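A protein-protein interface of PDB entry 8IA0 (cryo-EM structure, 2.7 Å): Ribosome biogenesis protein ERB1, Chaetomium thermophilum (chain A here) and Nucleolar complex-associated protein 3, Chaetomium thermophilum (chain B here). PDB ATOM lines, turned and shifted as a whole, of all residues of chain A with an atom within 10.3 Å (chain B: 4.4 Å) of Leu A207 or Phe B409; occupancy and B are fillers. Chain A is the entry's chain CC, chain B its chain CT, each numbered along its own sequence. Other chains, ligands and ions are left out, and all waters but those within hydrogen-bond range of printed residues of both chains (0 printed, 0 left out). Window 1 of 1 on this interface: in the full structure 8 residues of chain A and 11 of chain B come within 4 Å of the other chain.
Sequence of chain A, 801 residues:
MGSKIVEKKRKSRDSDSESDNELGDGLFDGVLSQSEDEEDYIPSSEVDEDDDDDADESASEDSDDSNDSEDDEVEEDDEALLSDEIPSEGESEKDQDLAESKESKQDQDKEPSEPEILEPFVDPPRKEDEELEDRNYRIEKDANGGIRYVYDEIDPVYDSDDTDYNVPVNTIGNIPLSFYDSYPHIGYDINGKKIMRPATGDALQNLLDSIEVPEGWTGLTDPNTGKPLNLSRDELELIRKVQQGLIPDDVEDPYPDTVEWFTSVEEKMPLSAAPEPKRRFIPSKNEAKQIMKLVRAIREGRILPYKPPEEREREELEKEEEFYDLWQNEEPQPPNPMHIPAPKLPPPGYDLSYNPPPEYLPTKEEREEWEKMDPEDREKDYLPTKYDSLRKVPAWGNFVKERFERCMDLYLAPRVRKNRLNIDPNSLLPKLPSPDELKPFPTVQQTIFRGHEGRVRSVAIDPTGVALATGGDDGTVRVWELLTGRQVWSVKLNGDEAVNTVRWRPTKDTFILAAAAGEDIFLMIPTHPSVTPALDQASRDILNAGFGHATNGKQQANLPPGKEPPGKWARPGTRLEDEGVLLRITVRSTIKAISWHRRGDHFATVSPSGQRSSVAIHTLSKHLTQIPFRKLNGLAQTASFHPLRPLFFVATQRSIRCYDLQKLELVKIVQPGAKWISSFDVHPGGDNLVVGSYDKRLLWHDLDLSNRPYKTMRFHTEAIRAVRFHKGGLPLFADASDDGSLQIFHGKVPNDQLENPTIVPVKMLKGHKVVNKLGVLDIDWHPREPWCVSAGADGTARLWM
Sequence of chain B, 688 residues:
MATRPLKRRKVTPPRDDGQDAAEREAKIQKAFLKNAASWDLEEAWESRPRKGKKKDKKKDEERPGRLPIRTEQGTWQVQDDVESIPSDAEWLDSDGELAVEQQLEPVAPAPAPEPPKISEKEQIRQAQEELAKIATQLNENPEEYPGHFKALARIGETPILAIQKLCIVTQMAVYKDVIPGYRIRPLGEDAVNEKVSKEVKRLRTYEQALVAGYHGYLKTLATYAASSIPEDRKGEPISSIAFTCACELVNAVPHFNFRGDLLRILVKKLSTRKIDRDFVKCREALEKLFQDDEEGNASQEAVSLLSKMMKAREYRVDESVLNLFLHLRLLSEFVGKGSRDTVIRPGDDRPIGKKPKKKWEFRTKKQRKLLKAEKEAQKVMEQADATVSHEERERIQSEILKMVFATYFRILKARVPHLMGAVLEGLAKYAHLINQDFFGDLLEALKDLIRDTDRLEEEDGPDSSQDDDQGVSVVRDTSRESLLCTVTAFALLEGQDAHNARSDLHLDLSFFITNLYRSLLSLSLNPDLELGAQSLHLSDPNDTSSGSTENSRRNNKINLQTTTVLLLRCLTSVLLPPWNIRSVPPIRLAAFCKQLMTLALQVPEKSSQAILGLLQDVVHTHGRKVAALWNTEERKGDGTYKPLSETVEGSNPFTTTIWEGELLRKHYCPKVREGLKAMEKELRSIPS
Ala A203 touches Ala B445 (CB to CA, 3.9 Å). CD1 of Leu A204 touches CB of Leu B412, at 3.6 Å. N of Lys B413 touches CD1 of Leu A204, 3.7 Å away. CD2 of Leu A204 touches CB of Ala B445 (3.9 Å). Lys B413 touches Gln A205 (CD to OE1, 3.6 Å). CE2 of Phe B409 touches CB of Leu A207 (3.7 Å). Leu A207 touches Asp B441. CD1 of Leu A207 touches CB of Ala B445, 3.7 Å away. O of Ala B406 touches CD2 of Leu A208, 3.9 Å away. Ile A211 touches Phe B405 (CD1 to CB, 3.5 Å).
Of the 13 printed residues of chain B, 8 touch a printed residue of chain A. Hydrophobic or aromatic side chains of chain B within 4 Å of the printed part of chain A: Phe B405, Phe B409, Leu B412 and Ala B445. Of the 14 printed residues of chain A, 7 touch a printed residue of chain B. Among the printed residues, 12 pairs touch across the chains.
The backbone carbonyl oxygen of Leu A207 sits at hydrogen-bond distance from the side-chain hydroxyl of Ser A210 (2.6 Å). The side-chain amide nitrogen of Gln A205 sits at hydrogen-bond distance from the side-chain carboxylate of Asp A209, 2.7 Å away.
Of chain B, only Phe B409 (3.7 Å), Asp B441 (3.8 Å) and Ala B445 (3.7 Å) come within 4 Å of Leu A207. Of the printed residues of chain B, Ile A211 touches Phe B405 and Phe B409. Of chain A, only Leu A207 and Ile A211 come within 4 Å of Phe B409. Of the printed residues of chain A, Arg B410 touches Glu A212 (3.1 Å). Printed residues of chain A within 4 Å of Leu B412: Leu A204 (3.6 Å). The nearest residue of chain B that does not touch Leu A207 is Leu B442 (4.1 Å). The nearest residue of chain A that does not touch Phe B409 is Leu A208 (4.04 Å).
NH2 of Arg B410 is in salt-bridge range of OE1 of Glu A212, 3.1 Å away.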
ATOM      1  N   GLY A 201      18.538  35.219 -11.425  1.00  0.00           N
ATOM      2  CA  GLY A 201      18.471  33.891 -10.861  1.00  0.00           C
ATOM      3  C   GLY A 201      17.050  33.368 -10.787  1.00  0.00           C
ATOM      4  O   GLY A 201      16.073  34.117 -10.813  1.00  0.00           O
ATOM      5  N   ASP A 202      16.940  32.047 -10.697  1.00  0.00           N
ATOM      6  CA  ASP A 202      15.634  31.412 -10.620  1.00  0.00           C
ATOM      7  C   ASP A 202      14.940  31.766  -9.311  1.00  0.00           C
ATOM      8  O   ASP A 202      15.581  32.004  -8.284  1.00  0.00           O
ATOM      9  CB  ASP A 202      15.770  29.895 -10.744  1.00  0.00           C
ATOM     10  CG  ASP A 202      16.749  29.484 -11.825  1.00  0.00           C
ATOM     11  OD1 ASP A 202      16.934  30.258 -12.787  1.00  0.00           O
ATOM     12  OD2 ASP A 202      17.334  28.386 -11.712  1.00  0.00           O
ATOM     13  N   ALA A 203      13.606  31.807  -9.359  1.00  0.00           N
ATOM     14  CA  ALA A 203      12.834  32.069  -8.150  1.00  0.00           C
ATOM     15  C   ALA A 203      13.025  30.958  -7.128  1.00  0.00           C
ATOM     16  O   ALA A 203      13.037  31.212  -5.918  1.00  0.00           O
ATOM     17  CB  ALA A 203      11.355  32.233  -8.491  1.00  0.00           C
ATOM     18  N   LEU A 204      13.169  29.718  -7.596  1.00  0.00           N
ATOM     19  CA  LEU A 204      13.382  28.599  -6.684  1.00  0.00           C
ATOM     20  C   LEU A 204      14.720  28.718  -5.968  1.00  0.00           C
ATOM     21  O   LEU A 204      14.826  28.399  -4.779  1.00  0.00           O
ATOM     22  CB  LEU A 204      13.295  27.281  -7.446  1.00  0.00           C
ATOM     23  CG  LEU A 204      11.881  26.845  -7.831  1.00  0.00           C
ATOM     24  CD1 LEU A 204      11.927  25.606  -8.705  1.00  0.00           C
ATOM     25  CD2 LEU A 204      11.041  26.601  -6.590  1.00  0.00           C
ATOM     26  N   GLN A 205      15.756  29.168  -6.678  1.00  0.00           N
ATOM     27  CA  GLN A 205      17.061  29.336  -6.051  1.00  0.00           C
ATOM     28  C   GLN A 205      17.019  30.414  -4.977  1.00  0.00           C
ATOM     29  O   GLN A 205      17.671  30.287  -3.934  1.00  0.00           O
ATOM     30  CB  GLN A 205      18.112  29.669  -7.109  1.00  0.00           C
ATOM     31  CG  GLN A 205      19.528  29.755  -6.568  1.00  0.00           C
ATOM     32  CD  GLN A 205      19.988  28.459  -5.934  1.00  0.00           C
ATOM     33  OE1 GLN A 205      19.810  27.381  -6.499  1.00  0.00           O
ATOM     34  NE2 GLN A 205      20.585  28.557  -4.753  1.00  0.00           N
ATOM     35  N   ASN A 206      16.261  31.487  -5.217  1.00  0.00           N
ATOM     36  CA  ASN A 206      16.115  32.528  -4.205  1.00  0.00           C
ATOM     37  C   ASN A 206      15.435  31.989  -2.955  1.00  0.00           C
ATOM     38  O   ASN A 206      15.825  32.326  -1.832  1.00  0.00           O
ATOM     39  CB  ASN A 206      15.329  33.707  -4.775  1.00  0.00           C
ATOM     40  CG  ASN A 206      16.207  34.685  -5.521  1.00  0.00           C
ATOM     41  OD1 ASN A 206      16.448  34.531  -6.718  1.00  0.00           O
ATOM     42  ND2 ASN A 206      16.693  35.699  -4.818  1.00  0.00           N
ATOM     43  N   LEU A 207      14.409  31.154  -3.129  1.00  0.00           N
ATOM     44  CA  LEU A 207      13.733  30.565  -1.980  1.00  0.00           C
ATOM     45  C   LEU A 207      14.667  29.643  -1.206  1.00  0.00           C
ATOM     46  O   LEU A 207      14.639  29.614   0.030  1.00  0.00           O
ATOM     47  CB  LEU A 207      12.487  29.808  -2.436  1.00  0.00           C
ATOM     48  CG  LEU A 207      11.197  30.627  -2.500  1.00  0.00           C
ATOM     49  CD1 LEU A 207      10.171  29.932  -3.372  1.00  0.00           C
ATOM     50  CD2 LEU A 207      10.646  30.868  -1.107  1.00  0.00           C
ATOM     51  N   LEU A 208      15.496  28.877  -1.916  1.00  0.00           N
ATOM     52  CA  LEU A 208      16.469  28.024  -1.246  1.00  0.00           C
ATOM     53  C   LEU A 208      17.477  28.849  -0.459  1.00  0.00           C
ATOM     54  O   LEU A 208      17.833  28.494   0.670  1.00  0.00           O
ATOM     55  CB  LEU A 208      17.186  27.143  -2.268  1.00  0.00           C
ATOM     56  CG  LEU A 208      16.693  25.703  -2.375  1.00  0.00           C
ATOM     57  CD1 LEU A 208      17.524  24.933  -3.385  1.00  0.00           C
ATOM     58  CD2 LEU A 208      16.733  25.027  -1.016  1.00  0.00           C
ATOM     59  N   ASP A 209      17.949  29.953  -1.041  1.00  0.00           N
ATOM     60  CA  ASP A 209      18.906  30.803  -0.341  1.00  0.00           C
ATOM     61  C   ASP A 209      18.282  31.429   0.899  1.00  0.00           C
ATOM     62  O   ASP A 209      18.946  31.576   1.931  1.00  0.00           O
ATOM     63  CB  ASP A 209      19.435  31.883  -1.282  1.00  0.00           C
ATOM     64  CG  ASP A 209      20.224  31.309  -2.440  1.00  0.00           C
ATOM     65  OD1 ASP A 209      20.299  30.067  -2.554  1.00  0.00           O
ATOM     66  OD2 ASP A 209      20.772  32.099  -3.239  1.00  0.00           O
ATOM     67  N   SER A 210      17.006  31.811   0.814  1.00  0.00           N
ATOM     68  CA  SER A 210      16.331  32.391   1.970  1.00  0.00           C
ATOM     69  C   SER A 210      16.181  31.374   3.094  1.00  0.00           C
ATOM     70  O   SER A 210      16.372  31.704   4.269  1.00  0.00           O
ATOM     71  CB  SER A 210      14.968  32.941   1.557  1.00  0.00           C
ATOM     72  OG  SER A 210      14.099  31.895   1.153  1.00  0.00           O
ATOM     73  N   ILE A 211      15.836  30.131   2.754  1.00  0.00           N
ATOM     74  CA  ILE A 211      15.619  29.111   3.776  1.00  0.00           C
ATOM     75  C   ILE A 211      16.936  28.724   4.436  1.00  0.00           C
ATOM     76  O   ILE A 211      17.041  28.673   5.667  1.00  0.00           O
ATOM     77  CB  ILE A 211      14.910  27.889   3.167  1.00  0.00           C
ATOM     78  CG1 ILE A 211      13.415  28.162   3.043  1.00  0.00           C
ATOM     79  CG2 ILE A 211      15.154  26.652   4.008  1.00  0.00           C
ATOM     80  CD1 ILE A 211      12.647  27.007   2.489  1.00  0.00           C
ATOM     81  N   GLU A 212      17.958  28.447   3.634  1.00  0.00           N
ATOM     82  CA  GLU A 212      19.290  28.107   4.128  1.00  0.00           C
ATOM     83  C   GLU A 212      20.264  29.128   3.548  1.00  0.00           C
ATOM     84  O   GLU A 212      20.613  29.079   2.367  1.00  0.00           O
ATOM     85  CB  GLU A 212      19.671  26.663   3.770  1.00  0.00           C
ATOM     86  CG  GLU A 212      19.413  26.263   2.327  1.00  0.00           C
ATOM     87  CD  GLU A 212      20.126  24.983   1.942  1.00  0.00           C
ATOM     88  OE1 GLU A 212      19.867  23.942   2.579  1.00  0.00           O
ATOM     89  OE2 GLU A 212      20.946  25.018   1.001  1.00  0.00           O
ATOM     90  N   VAL A 213      20.685  30.068   4.388  1.00  0.00           N
ATOM     91  CA  VAL A 213      21.541  31.157   3.911  1.00  0.00           C
ATOM     92  C   VAL A 213      22.881  30.590   3.468  1.00  0.00           C
ATOM     93  O   VAL A 213      23.414  29.675   4.128  1.00  0.00           O
ATOM     94  CB  VAL A 213      21.727  32.220   5.005  1.00  0.00           C
ATOM     95  CG1 VAL A 213      20.517  33.134   5.064  1.00  0.00           C
ATOM     96  CG2 VAL A 213      21.958  31.557   6.352  1.00  0.00           C
ATOM     97  N   PRO A 214      23.463  31.067   2.372  1.00  0.00           N
ATOM     98  CA  PRO A 214      24.793  30.595   1.980  1.00  0.00           C
ATOM     99  C   PRO A 214      25.839  30.996   3.007  1.00  0.00           C
ATOM    100  O   PRO A 214      25.627  31.876   3.844  1.00  0.00           O
ATOM    101  CB  PRO A 214      25.037  31.288   0.633  1.00  0.00           C
ATOM    102  CG  PRO A 214      23.677  31.648   0.139  1.00  0.00           C
ATOM    103  CD  PRO A 214      22.879  31.964   1.363  1.00  0.00           C
ATOM    104  N   PHE B 405      10.929  22.072   3.826  1.00  0.00           N
ATOM    105  CA  PHE B 405      10.767  22.987   2.703  1.00  0.00           C
ATOM    106  C   PHE B 405      11.995  23.008   1.801  1.00  0.00           C
ATOM    107  O   PHE B 405      11.865  23.222   0.591  1.00  0.00           O
ATOM    108  CB  PHE B 405      10.452  24.390   3.212  1.00  0.00           C
ATOM    109  CG  PHE B 405       8.987  24.679   3.318  1.00  0.00           C
ATOM    110  CD1 PHE B 405       8.272  24.292   4.435  1.00  0.00           C
ATOM    111  CD2 PHE B 405       8.323  25.338   2.303  1.00  0.00           C
ATOM    112  CE1 PHE B 405       6.925  24.556   4.533  1.00  0.00           C
ATOM    113  CE2 PHE B 405       6.977  25.605   2.399  1.00  0.00           C
ATOM    114  CZ  PHE B 405       6.277  25.213   3.513  1.00  0.00           C
ATOM    115  N   ALA B 406      13.190  22.804   2.361  1.00  0.00           N
ATOM    116  CA  ALA B 406      14.388  22.757   1.528  1.00  0.00           C
ATOM    117  C   ALA B 406      14.349  21.571   0.575  1.00  0.00           C
ATOM    118  O   ALA B 406      14.713  21.695  -0.600  1.00  0.00           O
ATOM    119  CB  ALA B 406      15.640  22.700   2.400  1.00  0.00           C
ATOM    120  N   THR B 407      13.911  20.410   1.065  1.00  0.00           N
ATOM    121  CA  THR B 407      13.764  19.247   0.198  1.00  0.00           C
ATOM    122  C   THR B 407      12.722  19.498  -0.883  1.00  0.00           C
ATOM    123  O   THR B 407      12.915  19.115  -2.042  1.00  0.00           O
ATOM    124  CB  THR B 407      13.392  18.019   1.032  1.00  0.00           C
ATOM    125  OG1 THR B 407      14.490  17.669   1.883  1.00  0.00           O
ATOM    126  CG2 THR B 407      13.064  16.838   0.138  1.00  0.00           C
ATOM    127  N   TYR B 408      11.619  20.157  -0.525  1.00  0.00           N
ATOM    128  CA  TYR B 408      10.565  20.437  -1.495  1.00  0.00           C
ATOM    129  C   TYR B 408      11.091  21.278  -2.650  1.00  0.00           C
ATOM    130  O   TYR B 408      10.776  21.021  -3.817  1.00  0.00           O
ATOM    131  CB  TYR B 408       9.399  21.148  -0.809  1.00  0.00           C
ATOM    132  CG  TYR B 408       8.480  20.232  -0.039  1.00  0.00           C
ATOM    133  CD1 TYR B 408       8.512  18.860  -0.237  1.00  0.00           C
ATOM    134  CD2 TYR B 408       7.579  20.739   0.881  1.00  0.00           C
ATOM    135  CE1 TYR B 408       7.675  18.022   0.462  1.00  0.00           C
ATOM    136  CE2 TYR B 408       6.738  19.909   1.586  1.00  0.00           C
ATOM    137  CZ  TYR B 408       6.790  18.552   1.374  1.00  0.00           C
ATOM    138  OH  TYR B 408       5.951  17.719   2.077  1.00  0.00           O
ATOM    139  N   PHE B 409      11.899  22.292  -2.341  1.00  0.00           N
ATOM    140  CA  PHE B 409      12.361  23.206  -3.379  1.00  0.00           C
ATOM    141  C   PHE B 409      13.448  22.576  -4.240  1.00  0.00           C
ATOM    142  O   PHE B 409      13.521  22.842  -5.444  1.00  0.00           O
ATOM    143  CB  PHE B 409      12.856  24.503  -2.749  1.00  0.00           C
ATOM    144  CG  PHE B 409      11.766  25.326  -2.132  1.00  0.00           C
ATOM    145  CD1 PHE B 409      10.457  25.180  -2.543  1.00  0.00           C
ATOM    146  CD2 PHE B 409      12.052  26.247  -1.144  1.00  0.00           C
ATOM    147  CE1 PHE B 409       9.455  25.934  -1.980  1.00  0.00           C
ATOM    148  CE2 PHE B 409      11.054  27.004  -0.581  1.00  0.00           C
ATOM    149  CZ  PHE B 409       9.755  26.846  -0.996  1.00  0.00           C
ATOM    150  N   ARG B 410      14.305  21.745  -3.645  1.00  0.00           N
ATOM    151  CA  ARG B 410      15.370  21.123  -4.423  1.00  0.00           C
ATOM    152  C   ARG B 410      14.809  20.103  -5.406  1.00  0.00           C
ATOM    153  O   ARG B 410      15.398  19.863  -6.466  1.00  0.00           O
ATOM    154  CB  ARG B 410      16.399  20.480  -3.493  1.00  0.00           C
ATOM    155  CG  ARG B 410      17.833  20.889  -3.796  1.00  0.00           C
ATOM    156  CD  ARG B 410      18.829  20.245  -2.844  1.00  0.00           C
ATOM    157  NE  ARG B 410      18.608  20.626  -1.455  1.00  0.00           N
ATOM    158  CZ  ARG B 410      19.321  21.538  -0.808  1.00  0.00           C
ATOM    159  NH1 ARG B 410      20.314  22.183  -1.396  1.00  0.00           N
ATOM    160  NH2 ARG B 410      19.031  21.807   0.461  1.00  0.00           N
ATOM    161  N   ILE B 411      13.673  19.487  -5.073  1.00  0.00           N
ATOM    162  CA  ILE B 411      12.998  18.615  -6.029  1.00  0.00           C
ATOM    163  C   ILE B 411      12.416  19.435  -7.169  1.00  0.00           C
ATOM    164  O   ILE B 411      12.485  19.040  -8.340  1.00  0.00           O
ATOM    165  CB  ILE B 411      11.914  17.780  -5.322  1.00  0.00           C
ATOM    166  CG1 ILE B 411      12.542  16.900  -4.243  1.00  0.00           C
ATOM    167  CG2 ILE B 411      11.155  16.930  -6.324  1.00  0.00           C
ATOM    168  CD1 ILE B 411      11.542  16.120  -3.429  1.00  0.00           C
ATOM    169  N   LEU B 412      11.830  20.589  -6.846  1.00  0.00           N
ATOM    170  CA  LEU B 412      11.271  21.453  -7.877  1.00  0.00           C
ATOM    171  C   LEU B 412      12.354  21.963  -8.819  1.00  0.00           C
ATOM    172  O   LEU B 412      12.146  22.030 -10.036  1.00  0.00           O
ATOM    173  CB  LEU B 412      10.530  22.621  -7.230  1.00  0.00           C
ATOM    174  CG  LEU B 412       9.204  22.320  -6.530  1.00  0.00           C
ATOM    175  CD1 LEU B 412       8.487  23.609  -6.181  1.00  0.00           C
ATOM    176  CD2 LEU B 412       8.324  21.438  -7.392  1.00  0.00           C
ATOM    177  N   LYS B 413      13.514  22.339  -8.275  1.00  0.00           N
ATOM    178  CA  LYS B 413      14.591  22.850  -9.116  1.00  0.00           C
ATOM    179  C   LYS B 413      15.117  21.777 -10.060  1.00  0.00           C
ATOM    180  O   LYS B 413      15.370  22.051 -11.238  1.00  0.00           O
ATOM    181  CB  LYS B 413      15.721  23.403  -8.249  1.00  0.00           C
ATOM    182  CG  LYS B 413      16.814  24.098  -9.039  1.00  0.00           C
ATOM    183  CD  LYS B 413      17.782  24.825  -8.129  1.00  0.00           C
ATOM    184  CE  LYS B 413      18.659  23.848  -7.369  1.00  0.00           C
ATOM    185  NZ  LYS B 413      19.602  23.134  -8.274  1.00  0.00           N
ATOM    186  N   LEU B 427       3.599  21.684  -0.216  1.00  0.00           N
ATOM    187  CA  LEU B 427       3.652  23.142  -0.207  1.00  0.00           C
ATOM    188  C   LEU B 427       2.283  23.733   0.093  1.00  0.00           C
ATOM    189  O   LEU B 427       2.159  24.678   0.878  1.00  0.00           O
ATOM    190  CB  LEU B 427       4.176  23.662  -1.545  1.00  0.00           C
ATOM    191  CG  LEU B 427       5.667  23.486  -1.822  1.00  0.00           C
ATOM    192  CD1 LEU B 427       6.003  23.939  -3.232  1.00  0.00           C
ATOM    193  CD2 LEU B 427       6.486  24.254  -0.804  1.00  0.00           C
ATOM    194  N   ASP B 441       6.423  34.640  -2.448  1.00  0.00           N
ATOM    195  CA  ASP B 441       7.485  34.006  -3.222  1.00  0.00           C
ATOM    196  C   ASP B 441       7.041  32.656  -3.769  1.00  0.00           C
ATOM    197  O   ASP B 441       7.451  32.257  -4.865  1.00  0.00           O
ATOM    198  CB  ASP B 441       8.737  33.847  -2.363  1.00  0.00           C
ATOM    199  CG  ASP B 441       9.180  35.148  -1.735  1.00  0.00           C
ATOM    200  OD1 ASP B 441       8.613  36.202  -2.089  1.00  0.00           O
ATOM    201  OD2 ASP B 441      10.097  35.120  -0.887  1.00  0.00           O
ATOM    202  N   LEU B 442       6.214  31.931  -3.013  1.00  0.00           N
ATOM    203  CA  LEU B 442       5.738  30.633  -3.477  1.00  0.00           C
ATOM    204  C   LEU B 442       4.909  30.771  -4.746  1.00  0.00           C
ATOM    205  O   LEU B 442       5.039  29.962  -5.671  1.00  0.00           O
ATOM    206  CB  LEU B 442       4.926  29.947  -2.380  1.00  0.00           C
ATOM    207  CG  LEU B 442       5.683  29.597  -1.101  1.00  0.00           C
ATOM    208  CD1 LEU B 442       4.737  29.042  -0.055  1.00  0.00           C
ATOM    209  CD2 LEU B 442       6.789  28.607  -1.399  1.00  0.00           C
ATOM    210  N   ALA B 445       7.321  31.497  -7.548  1.00  0.00           N
ATOM    211  CA  ALA B 445       8.017  30.274  -7.935  1.00  0.00           C
ATOM    212  C   ALA B 445       7.121  29.372  -8.774  1.00  0.00           C
ATOM    213  O   ALA B 445       7.595  28.708  -9.703  1.00  0.00           O
ATOM    214  CB  ALA B 445       8.512  29.535  -6.694  1.00  0.00           C
